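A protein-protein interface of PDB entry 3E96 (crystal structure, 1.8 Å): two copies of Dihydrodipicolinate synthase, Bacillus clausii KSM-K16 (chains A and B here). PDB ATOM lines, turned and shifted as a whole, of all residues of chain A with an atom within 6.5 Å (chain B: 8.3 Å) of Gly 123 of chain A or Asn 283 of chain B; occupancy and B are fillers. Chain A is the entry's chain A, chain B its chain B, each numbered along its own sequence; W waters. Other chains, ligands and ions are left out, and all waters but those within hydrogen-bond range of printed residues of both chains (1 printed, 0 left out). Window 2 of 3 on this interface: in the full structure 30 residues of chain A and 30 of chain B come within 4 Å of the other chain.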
ATOM      1  N   THR A 121      31.202 -10.816 -17.846  1.00  0.00           N
ATOM      2  CA  THR A 121      30.893 -12.241 -17.795  1.00  0.00           C
ATOM      3  C   THR A 121      29.491 -12.381 -18.373  1.00  0.00           C
ATOM      4  O   THR A 121      28.723 -11.414 -18.386  1.00  0.00           O
ATOM      5  CB  THR A 121      30.933 -12.817 -16.356  1.00  0.00           C
ATOM      6  OG1 THR A 121      29.988 -12.132 -15.529  1.00  0.00           O
ATOM      7  CG2 THR A 121      32.331 -12.673 -15.770  1.00  0.00           C
ATOM      8  N   ALA A 122      29.161 -13.572 -18.861  1.00  0.00           N
ATOM      9  CA  ALA A 122      27.856 -13.803 -19.470  1.00  0.00           C
ATOM     10  C   ALA A 122      26.695 -13.378 -18.571  1.00  0.00           C
ATOM     11  O   ALA A 122      25.795 -12.654 -19.004  1.00  0.00           O
ATOM     12  CB  ALA A 122      27.717 -15.277 -19.851  1.00  0.00           C
ATOM     13  N   GLY A 123      26.720 -13.825 -17.320  1.00  0.00           N
ATOM     14  CA  GLY A 123      25.652 -13.473 -16.396  1.00  0.00           C
ATOM     15  C   GLY A 123      25.555 -11.976 -16.172  1.00  0.00           C
ATOM     16  O   GLY A 123      24.457 -11.429 -16.038  1.00  0.00           O
ATOM     17  N   GLY A 124      26.706 -11.308 -16.140  1.00  0.00           N
ATOM     18  CA  GLY A 124      26.725  -9.871 -15.934  1.00  0.00           C
ATOM     19  C   GLY A 124      26.243  -9.091 -17.147  1.00  0.00           C
ATOM     20  O   GLY A 124      25.570  -8.069 -17.010  1.00  0.00           O
ATOM     21  N   VAL A 125      26.594  -9.563 -18.339  1.00  0.00           N
ATOM     22  CA  VAL A 125      26.176  -8.895 -19.570  1.00  0.00           C
ATOM     23  C   VAL A 125      24.664  -9.001 -19.705  1.00  0.00           C
ATOM     24  O   VAL A 125      24.002  -8.053 -20.112  1.00  0.00           O
ATOM     25  CB  VAL A 125      26.865  -9.520 -20.803  1.00  0.00           C
ATOM     26  CG1 VAL A 125      26.326  -8.885 -22.086  1.00  0.00           C
ATOM     27  CG2 VAL A 125      28.376  -9.306 -20.702  1.00  0.00           C
ATOM     28  N   TYR A 126      24.119 -10.163 -19.363  1.00  0.00           N
ATOM     29  CA  TYR A 126      22.679 -10.346 -19.418  1.00  0.00           C
ATOM     30  C   TYR A 126      22.021  -9.295 -18.515  1.00  0.00           C
ATOM     31  O   TYR A 126      21.111  -8.580 -18.930  1.00  0.00           O
ATOM     32  CB  TYR A 126      22.304 -11.744 -18.927  1.00  0.00           C
ATOM     33  CG  TYR A 126      20.827 -11.891 -18.668  1.00  0.00           C
ATOM     34  CD1 TYR A 126      19.924 -12.024 -19.720  1.00  0.00           C
ATOM     35  CD2 TYR A 126      20.325 -11.843 -17.369  1.00  0.00           C
ATOM     36  CE1 TYR A 126      18.554 -12.106 -19.485  1.00  0.00           C
ATOM     37  CE2 TYR A 126      18.961 -11.921 -17.123  1.00  0.00           C
ATOM     38  CZ  TYR A 126      18.083 -12.052 -18.182  1.00  0.00           C
ATOM     39  OH  TYR A 126      16.733 -12.120 -17.933  1.00  0.00           O
ATOM     40  N   ALA A 127      22.500  -9.205 -17.279  1.00  0.00           N
ATOM     41  CA  ALA A 127      21.954  -8.254 -16.319  1.00  0.00           C
ATOM     42  C   ALA A 127      22.110  -6.813 -16.801  1.00  0.00           C
ATOM     43  O   ALA A 127      21.202  -5.997 -16.638  1.00  0.00           O
ATOM     44  CB  ALA A 127      22.641  -8.431 -14.965  1.00  0.00           C
ATOM     45  N   TYR A 128      23.259  -6.506 -17.402  1.00  0.00           N
ATOM     46  CA  TYR A 128      23.528  -5.152 -17.898  1.00  0.00           C
ATOM     47  C   TYR A 128      22.459  -4.707 -18.901  1.00  0.00           C
ATOM     48  O   TYR A 128      21.824  -3.662 -18.728  1.00  0.00           O
ATOM     49  CB  TYR A 128      24.908  -5.096 -18.564  1.00  0.00           C
ATOM     50  CG  TYR A 128      25.238  -3.747 -19.176  1.00  0.00           C
ATOM     51  CD1 TYR A 128      25.680  -2.685 -18.389  1.00  0.00           C
ATOM     52  CD2 TYR A 128      25.079  -3.531 -20.545  1.00  0.00           C
ATOM     53  CE1 TYR A 128      25.959  -1.438 -18.953  1.00  0.00           C
ATOM     54  CE2 TYR A 128      25.346  -2.303 -21.117  1.00  0.00           C
ATOM     55  CZ  TYR A 128      25.784  -1.259 -20.324  1.00  0.00           C
ATOM     56  OH  TYR A 128      26.037  -0.045 -20.911  1.00  0.00           O
ATOM     57  N   ILE A 149      31.445 -13.993 -24.893  1.00  0.00           N
ATOM     58  CA  ILE A 149      30.172 -14.021 -24.179  1.00  0.00           C
ATOM     59  C   ILE A 149      29.198 -14.932 -24.919  1.00  0.00           C
ATOM     60  O   ILE A 149      28.929 -14.736 -26.103  1.00  0.00           O
ATOM     61  CB  ILE A 149      29.559 -12.603 -24.068  1.00  0.00           C
ATOM     62  CG1 ILE A 149      30.503 -11.688 -23.278  1.00  0.00           C
ATOM     63  CG2 ILE A 149      28.175 -12.674 -23.400  1.00  0.00           C
ATOM     64  CD1 ILE A 149      30.679 -12.086 -21.814  1.00  0.00           C
ATOM     65  N   VAL A 153      23.011 -15.428 -23.714  1.00  0.00           N
ATOM     66  CA  VAL A 153      22.589 -14.117 -23.218  1.00  0.00           C
ATOM     67  C   VAL A 153      21.442 -13.592 -24.087  1.00  0.00           C
ATOM     68  O   VAL A 153      20.461 -13.039 -23.581  1.00  0.00           O
ATOM     69  CB  VAL A 153      23.757 -13.080 -23.261  1.00  0.00           C
ATOM     70  CG1 VAL A 153      23.224 -11.674 -23.000  1.00  0.00           C
ATOM     71  CG2 VAL A 153      24.821 -13.439 -22.222  1.00  0.00           C
ATOM     72  N   GLU B  58      36.412  -0.794 -10.846  1.00  0.00           N
ATOM     73  CA  GLU B  58      35.263  -0.884 -11.748  1.00  0.00           C
ATOM     74  C   GLU B  58      34.852   0.506 -12.237  1.00  0.00           C
ATOM     75  O   GLU B  58      33.677   0.869 -12.262  1.00  0.00           O
ATOM     76  CB  GLU B  58      34.094  -1.596 -11.067  1.00  0.00           C
ATOM     77  CG  GLU B  58      34.353  -3.079 -10.853  1.00  0.00           C
ATOM     78  CD  GLU B  58      33.232  -3.769 -10.108  1.00  0.00           C
ATOM     79  OE1 GLU B  58      32.229  -4.156 -10.752  1.00  0.00           O
ATOM     80  OE2 GLU B  58      33.351  -3.911  -8.867  1.00  0.00           O
ATOM     81  N   GLY B 258      37.203 -11.682 -16.950  1.00  0.00           N
ATOM     82  CA  GLY B 258      35.887 -11.367 -16.419  1.00  0.00           C
ATOM     83  C   GLY B 258      35.834 -11.533 -14.907  1.00  0.00           C
ATOM     84  O   GLY B 258      35.072 -10.850 -14.226  1.00  0.00           O
ATOM     85  N   ASN B 259      36.656 -12.442 -14.386  1.00  0.00           N
ATOM     86  CA  ASN B 259      36.720 -12.734 -12.949  1.00  0.00           C
ATOM     87  C   ASN B 259      37.614 -11.779 -12.158  1.00  0.00           C
ATOM     88  O   ASN B 259      37.671 -11.857 -10.929  1.00  0.00           O
ATOM     89  CB  ASN B 259      37.262 -14.151 -12.739  1.00  0.00           C
ATOM     90  CG  ASN B 259      36.172 -15.174 -12.500  1.00  0.00           C
ATOM     91  OD1 ASN B 259      34.997 -14.919 -12.748  1.00  0.00           O
ATOM     92  ND2 ASN B 259      36.567 -16.352 -12.020  1.00  0.00           N
ATOM     93  N   VAL B 261      37.703  -8.718 -10.813  1.00  0.00           N
ATOM     94  CA  VAL B 261      37.287  -8.052  -9.580  1.00  0.00           C
ATOM     95  C   VAL B 261      36.366  -8.904  -8.718  1.00  0.00           C
ATOM     96  O   VAL B 261      36.491  -8.918  -7.491  1.00  0.00           O
ATOM     97  CB  VAL B 261      36.574  -6.711  -9.888  1.00  0.00           C
ATOM     98  CG1 VAL B 261      36.049  -6.078  -8.591  1.00  0.00           C
ATOM     99  CG2 VAL B 261      37.540  -5.757 -10.586  1.00  0.00           C
ATOM    100  N   VAL B 262      35.443  -9.621  -9.350  1.00  0.00           N
ATOM    101  CA  VAL B 262      34.514 -10.436  -8.583  1.00  0.00           C
ATOM    102  C   VAL B 262      35.235 -11.467  -7.706  1.00  0.00           C
ATOM    103  O   VAL B 262      34.788 -11.746  -6.595  1.00  0.00           O
ATOM    104  CB  VAL B 262      33.463 -11.116  -9.500  1.00  0.00           C
ATOM    105  CG1 VAL B 262      34.135 -12.061 -10.477  1.00  0.00           C
ATOM    106  CG2 VAL B 262      32.423 -11.837  -8.643  1.00  0.00           C
ATOM    107  N   VAL B 263      36.349 -12.018  -8.184  1.00  0.00           N
ATOM    108  CA  VAL B 263      37.112 -12.982  -7.381  1.00  0.00           C
ATOM    109  C   VAL B 263      37.655 -12.276  -6.134  1.00  0.00           C
ATOM    110  O   VAL B 263      37.634 -12.831  -5.027  1.00  0.00           O
ATOM    111  CB  VAL B 263      38.301 -13.586  -8.175  1.00  0.00           C
ATOM    112  CG1 VAL B 263      39.246 -14.332  -7.230  1.00  0.00           C
ATOM    113  CG2 VAL B 263      37.776 -14.542  -9.240  1.00  0.00           C
ATOM    114  N   GLU B 266      34.617 -11.632  -3.639  1.00  0.00           N
ATOM    115  CA  GLU B 266      34.099 -12.806  -2.945  1.00  0.00           C
ATOM    116  C   GLU B 266      35.158 -13.385  -2.011  1.00  0.00           C
ATOM    117  O   GLU B 266      34.829 -13.988  -0.990  1.00  0.00           O
ATOM    118  CB  GLU B 266      33.588 -13.839  -3.949  1.00  0.00           C
ATOM    119  CG  GLU B 266      32.340 -13.339  -4.669  1.00  0.00           C
ATOM    120  CD  GLU B 266      31.494 -14.438  -5.274  1.00  0.00           C
ATOM    121  OE1 GLU B 266      31.591 -15.599  -4.816  1.00  0.00           O
ATOM    122  OE2 GLU B 266      30.712 -14.131  -6.200  1.00  0.00           O
ATOM    123  N   VAL B 277      29.321  -6.582  -3.734  1.00  0.00           N
ATOM    124  CA  VAL B 277      29.358  -7.270  -5.019  1.00  0.00           C
ATOM    125  C   VAL B 277      29.840  -6.387  -6.163  1.00  0.00           C
ATOM    126  O   VAL B 277      30.101  -5.197  -5.987  1.00  0.00           O
ATOM    127  CB  VAL B 277      27.956  -7.783  -5.405  1.00  0.00           C
ATOM    128  CG1 VAL B 277      27.458  -8.778  -4.373  1.00  0.00           C
ATOM    129  CG2 VAL B 277      26.991  -6.598  -5.517  1.00  0.00           C
ATOM    130  N   THR B 278      29.961  -6.990  -7.340  1.00  0.00           N
ATOM    131  CA  THR B 278      30.364  -6.254  -8.532  1.00  0.00           C
ATOM    132  C   THR B 278      29.080  -5.743  -9.178  1.00  0.00           C
ATOM    133  O   THR B 278      27.985  -6.192  -8.827  1.00  0.00           O
ATOM    134  CB  THR B 278      31.096  -7.164  -9.558  1.00  0.00           C
ATOM    135  OG1 THR B 278      30.324  -8.354  -9.790  1.00  0.00           O
ATOM    136  CG2 THR B 278      32.485  -7.543  -9.055  1.00  0.00           C
ATOM    137  N   ARG B 279      29.206  -4.791 -10.096  1.00  0.00           N
ATOM    138  CA  ARG B 279      28.047  -4.271 -10.813  1.00  0.00           C
ATOM    139  C   ARG B 279      28.031  -4.916 -12.198  1.00  0.00           C
ATOM    140  O   ARG B 279      29.083  -5.288 -12.724  1.00  0.00           O
ATOM    141  CB  ARG B 279      28.136  -2.751 -10.992  1.00  0.00           C
ATOM    142  CG  ARG B 279      27.620  -1.914  -9.824  1.00  0.00           C
ATOM    143  CD  ARG B 279      27.679  -0.425 -10.164  1.00  0.00           C
ATOM    144  NE  ARG B 279      27.191   0.415  -9.071  1.00  0.00           N
ATOM    145  CZ  ARG B 279      27.257   1.741  -9.053  1.00  0.00           C
ATOM    146  NH1 ARG B 279      26.790   2.415  -8.008  1.00  0.00           N
ATOM    147  NH2 ARG B 279      27.788   2.399 -10.075  1.00  0.00           N
ATOM    148  N   ALA B 280      26.845  -5.072 -12.777  1.00  0.00           N
ATOM    149  CA  ALA B 280      26.751  -5.617 -14.129  1.00  0.00           C
ATOM    150  C   ALA B 280      27.657  -4.652 -14.895  1.00  0.00           C
ATOM    151  O   ALA B 280      27.693  -3.467 -14.570  1.00  0.00           O
ATOM    152  CB  ALA B 280      25.315  -5.518 -14.640  1.00  0.00           C
ATOM    153  N   PRO B 281      28.336  -5.110 -15.961  1.00  0.00           N
ATOM    154  CA  PRO B 281      28.394  -6.428 -16.606  1.00  0.00           C
ATOM    155  C   PRO B 281      29.107  -7.624 -15.964  1.00  0.00           C
ATOM    156  O   PRO B 281      29.565  -8.515 -16.678  1.00  0.00           O
ATOM    157  CB  PRO B 281      28.976  -6.096 -17.975  1.00  0.00           C
ATOM    158  CG  PRO B 281      29.985  -5.039 -17.632  1.00  0.00           C
ATOM    159  CD  PRO B 281      29.213  -4.152 -16.663  1.00  0.00           C
ATOM    160  N   VAL B 282      29.228  -7.653 -14.642  1.00  0.00           N
ATOM    161  CA  VAL B 282      29.825  -8.817 -13.988  1.00  0.00           C
ATOM    162  C   VAL B 282      28.941  -9.182 -12.804  1.00  0.00           C
ATOM    163  O   VAL B 282      28.626  -8.326 -11.982  1.00  0.00           O
ATOM    164  CB  VAL B 282      31.264  -8.563 -13.477  1.00  0.00           C
ATOM    165  CG1 VAL B 282      31.732  -9.764 -12.642  1.00  0.00           C
ATOM    166  CG2 VAL B 282      32.214  -8.374 -14.659  1.00  0.00           C
ATOM    167  N   ASN B 283      28.519 -10.441 -12.729  1.00  0.00           N
ATOM    168  CA  ASN B 283      27.681 -10.869 -11.614  1.00  0.00           C
ATOM    169  C   ASN B 283      28.482 -11.791 -10.698  1.00  0.00           C
ATOM    170  O   ASN B 283      29.710 -11.846 -10.798  1.00  0.00           O
ATOM    171  CB  ASN B 283      26.387 -11.529 -12.126  1.00  0.00           C
ATOM    172  CG  ASN B 283      26.620 -12.858 -12.819  1.00  0.00           C
ATOM    173  OD1 ASN B 283      27.657 -13.085 -13.439  1.00  0.00           O
ATOM    174  ND2 ASN B 283      25.630 -13.742 -12.731  1.00  0.00           N
ATOM    175  N   GLU B 284      27.810 -12.508  -9.804  1.00  0.00           N
ATOM    176  CA  GLU B 284      28.529 -13.364  -8.861  1.00  0.00           C
ATOM    177  C   GLU B 284      29.175 -14.612  -9.445  1.00  0.00           C
ATOM    178  O   GLU B 284      28.857 -15.037 -10.554  1.00  0.00           O
ATOM    179  CB  GLU B 284      27.613 -13.755  -7.692  1.00  0.00           C
ATOM    180  CG  GLU B 284      26.465 -14.697  -8.036  1.00  0.00           C
ATOM    181  CD  GLU B 284      25.430 -14.077  -8.961  1.00  0.00           C
ATOM    182  OE1 GLU B 284      25.125 -12.872  -8.813  1.00  0.00           O
ATOM    183  OE2 GLU B 284      24.908 -14.804  -9.832  1.00  0.00           O
ATOM    184  N   LEU B 285      30.098 -15.195  -8.682  1.00  0.00           N
ATOM    185  CA  LEU B 285      30.805 -16.396  -9.110  1.00  0.00           C
ATOM    186  C   LEU B 285      29.894 -17.613  -9.125  1.00  0.00           C
ATOM    187  O   LEU B 285      28.914 -17.678  -8.383  1.00  0.00           O
ATOM    188  CB  LEU B 285      31.990 -16.686  -8.175  1.00  0.00           C
ATOM    189  CG  LEU B 285      33.173 -15.715  -8.160  1.00  0.00           C
ATOM    190  CD1 LEU B 285      34.213 -16.190  -7.149  1.00  0.00           C
ATOM    191  CD2 LEU B 285      33.787 -15.638  -9.551  1.00  0.00           C
ATOM    192  N   SER B 286      30.226 -18.576  -9.979  1.00  0.00           N
ATOM    193  CA  SER B 286      29.470 -19.821 -10.060  1.00  0.00           C
ATOM    194  C   SER B 286      29.866 -20.614  -8.818  1.00  0.00           C
ATOM    195  O   SER B 286      30.814 -20.243  -8.122  1.00  0.00           O
ATOM    196  CB  SER B 286      29.880 -20.609 -11.301  1.00  0.00           C
ATOM    197  OG  SER B 286      31.257 -20.951 -11.232  1.00  0.00           O
ATOM    198  N   LYS B 290      33.380 -20.433  -6.725  1.00  0.00           N
ATOM    199  CA  LYS B 290      33.327 -20.119  -5.296  1.00  0.00           C
ATOM    200  C   LYS B 290      34.169 -21.161  -4.553  1.00  0.00           C
ATOM    201  O   LYS B 290      34.872 -20.843  -3.594  1.00  0.00           O
ATOM    202  CB  LYS B 290      31.881 -20.159  -4.788  1.00  0.00           C
ATOM    203  CG  LYS B 290      31.081 -18.893  -5.054  1.00  0.00           C
ATOM    204  CD  LYS B 290      29.611 -19.100  -4.715  1.00  0.00           C
ATOM    205  CE  LYS B 290      28.877 -17.776  -4.532  1.00  0.00           C
ATOM    206  NZ  LYS B 290      29.071 -16.838  -5.673  1.00  0.00           N
HETATM  207  O   HOH W   1      30.541 -13.454 -12.920  1.00  0.00           O
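The backbone carbonyl oxygen (O) of Pro 281 of chain B sits at hydrogen-bond distance from the backbone NH (N) of Thr 121 of chain A.
The side-chain amide oxygen (OD1) of Asn 283 of chain B is in hydrogen-bond range of the side-chain hydroxyl (OG1) of Thr 121 of chain A.
The backbone NH (N) of Gly 124 of chain A sits at hydrogen-bond distance from the side-chain amide oxygen (OD1) of Asn 283 of chain B.
The backbone NH (N) of Gly 124 of chain A lies within hydrogen-bond range of the side-chain hydroxyl (OG1) of Thr 121 of chain A, 3.4 Å away.
The side-chain hydroxyl (OG1) of Thr 278 of chain B is in hydrogen-bond range of the backbone carbonyl oxygen (O) of Val 282 of chain B (2.8 Å).
ND2 of Asn 283 of chain B is in hydrogen-bond range of OE2 of Glu 284 of chain B (3.2 Å).
O of Gly 258 of chain B touches CG2 of Thr 121 of chain A (3.6 Å).
Thr 121 of chain A touches Val 282 of chain B (OG1 to CA, 3.7 Å).
Gly 123 of chain A touches Asn 283 of chain B.
Ala 280 of chain B touches Gly 124 of chain A.
Gly 124 of chain A touches Pro 281 of chain B (CA to O, 3.2 Å).
Val 282 of chain B touches Gly 124 of chain A (N to CA, 3.6 Å).
Pro 281 of chain B touches Val 125 of chain A (O to N, 3.6 Å).
Ala 280 of chain B touches Ala 127 of chain A.
N of Tyr 128 of chain A touches CB of Ala 280 of chain B, at 3.6 Å.
Printed residues of chain B within 4 Å of Gly 123 of chain A: Asn 283 (3.6 Å).
Asn 283 of chain B touches just these residues of chain A: Thr 121 (3.3 Å), Gly 123 (3.6 Å) and Gly 124 (3.4 Å).
Gly 124 of chain A touches four residues of chain B.
Of the printed residues of chain A, Ala 280 of chain B touches Gly 124 (3.5 Å), Ala 127 (3.97 Å) and Tyr 128 (3.6 Å).
Of the printed residues of chain B, Val 125 of chain A touches Pro 281 (3.6 Å).
Of the printed residues of chain A, Val 282 of chain B touches Thr 121 (3.7 Å) and Gly 124 (3.6 Å).
Of the printed residues of chain A, Pro 281 of chain B touches Thr 121 (3.1 Å), Gly 124 (3.2 Å) and Val 125 (3.6 Å).
Glu 58 of chain B touches none of the printed residues of chain A.
Ile 149 of chain A touches none of the printed residues of chain B.
The nearest residue of chain B that does not touch Gly 123 of chain A is Pro 281 of chain B (5.3 Å).
The nearest residue of chain A that does not touch Asn 283 of chain B is Ala 122 of chain A (5.2 Å).
Hydrophobic or aromatic side chains of chain B within 4 Å of the printed part of chain A: Ala 280.
Hydrophobic or aromatic side chains of chain A that line the printed part of chain B: Ala 127 and Tyr 128.
Among the printed residues, 12 pairs touch across the chains.
Among the printed residues, no Asp or Glu carboxylate lies within 4 Å of a Lys or Arg side-chain nitrogen of the other chain.
No position is printed for both chains.
Of the 12 pairs that touch across the chains among the printed residues, none has its exchanged pair printed and touching as well.
Water W1 lies within hydrogen-bond range of O of Asn 283 of chain B (2.8 Å), OG1 of Thr 121 of chain A (3.0 Å) and O of Glu 284 of chain B (3.3 Å).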
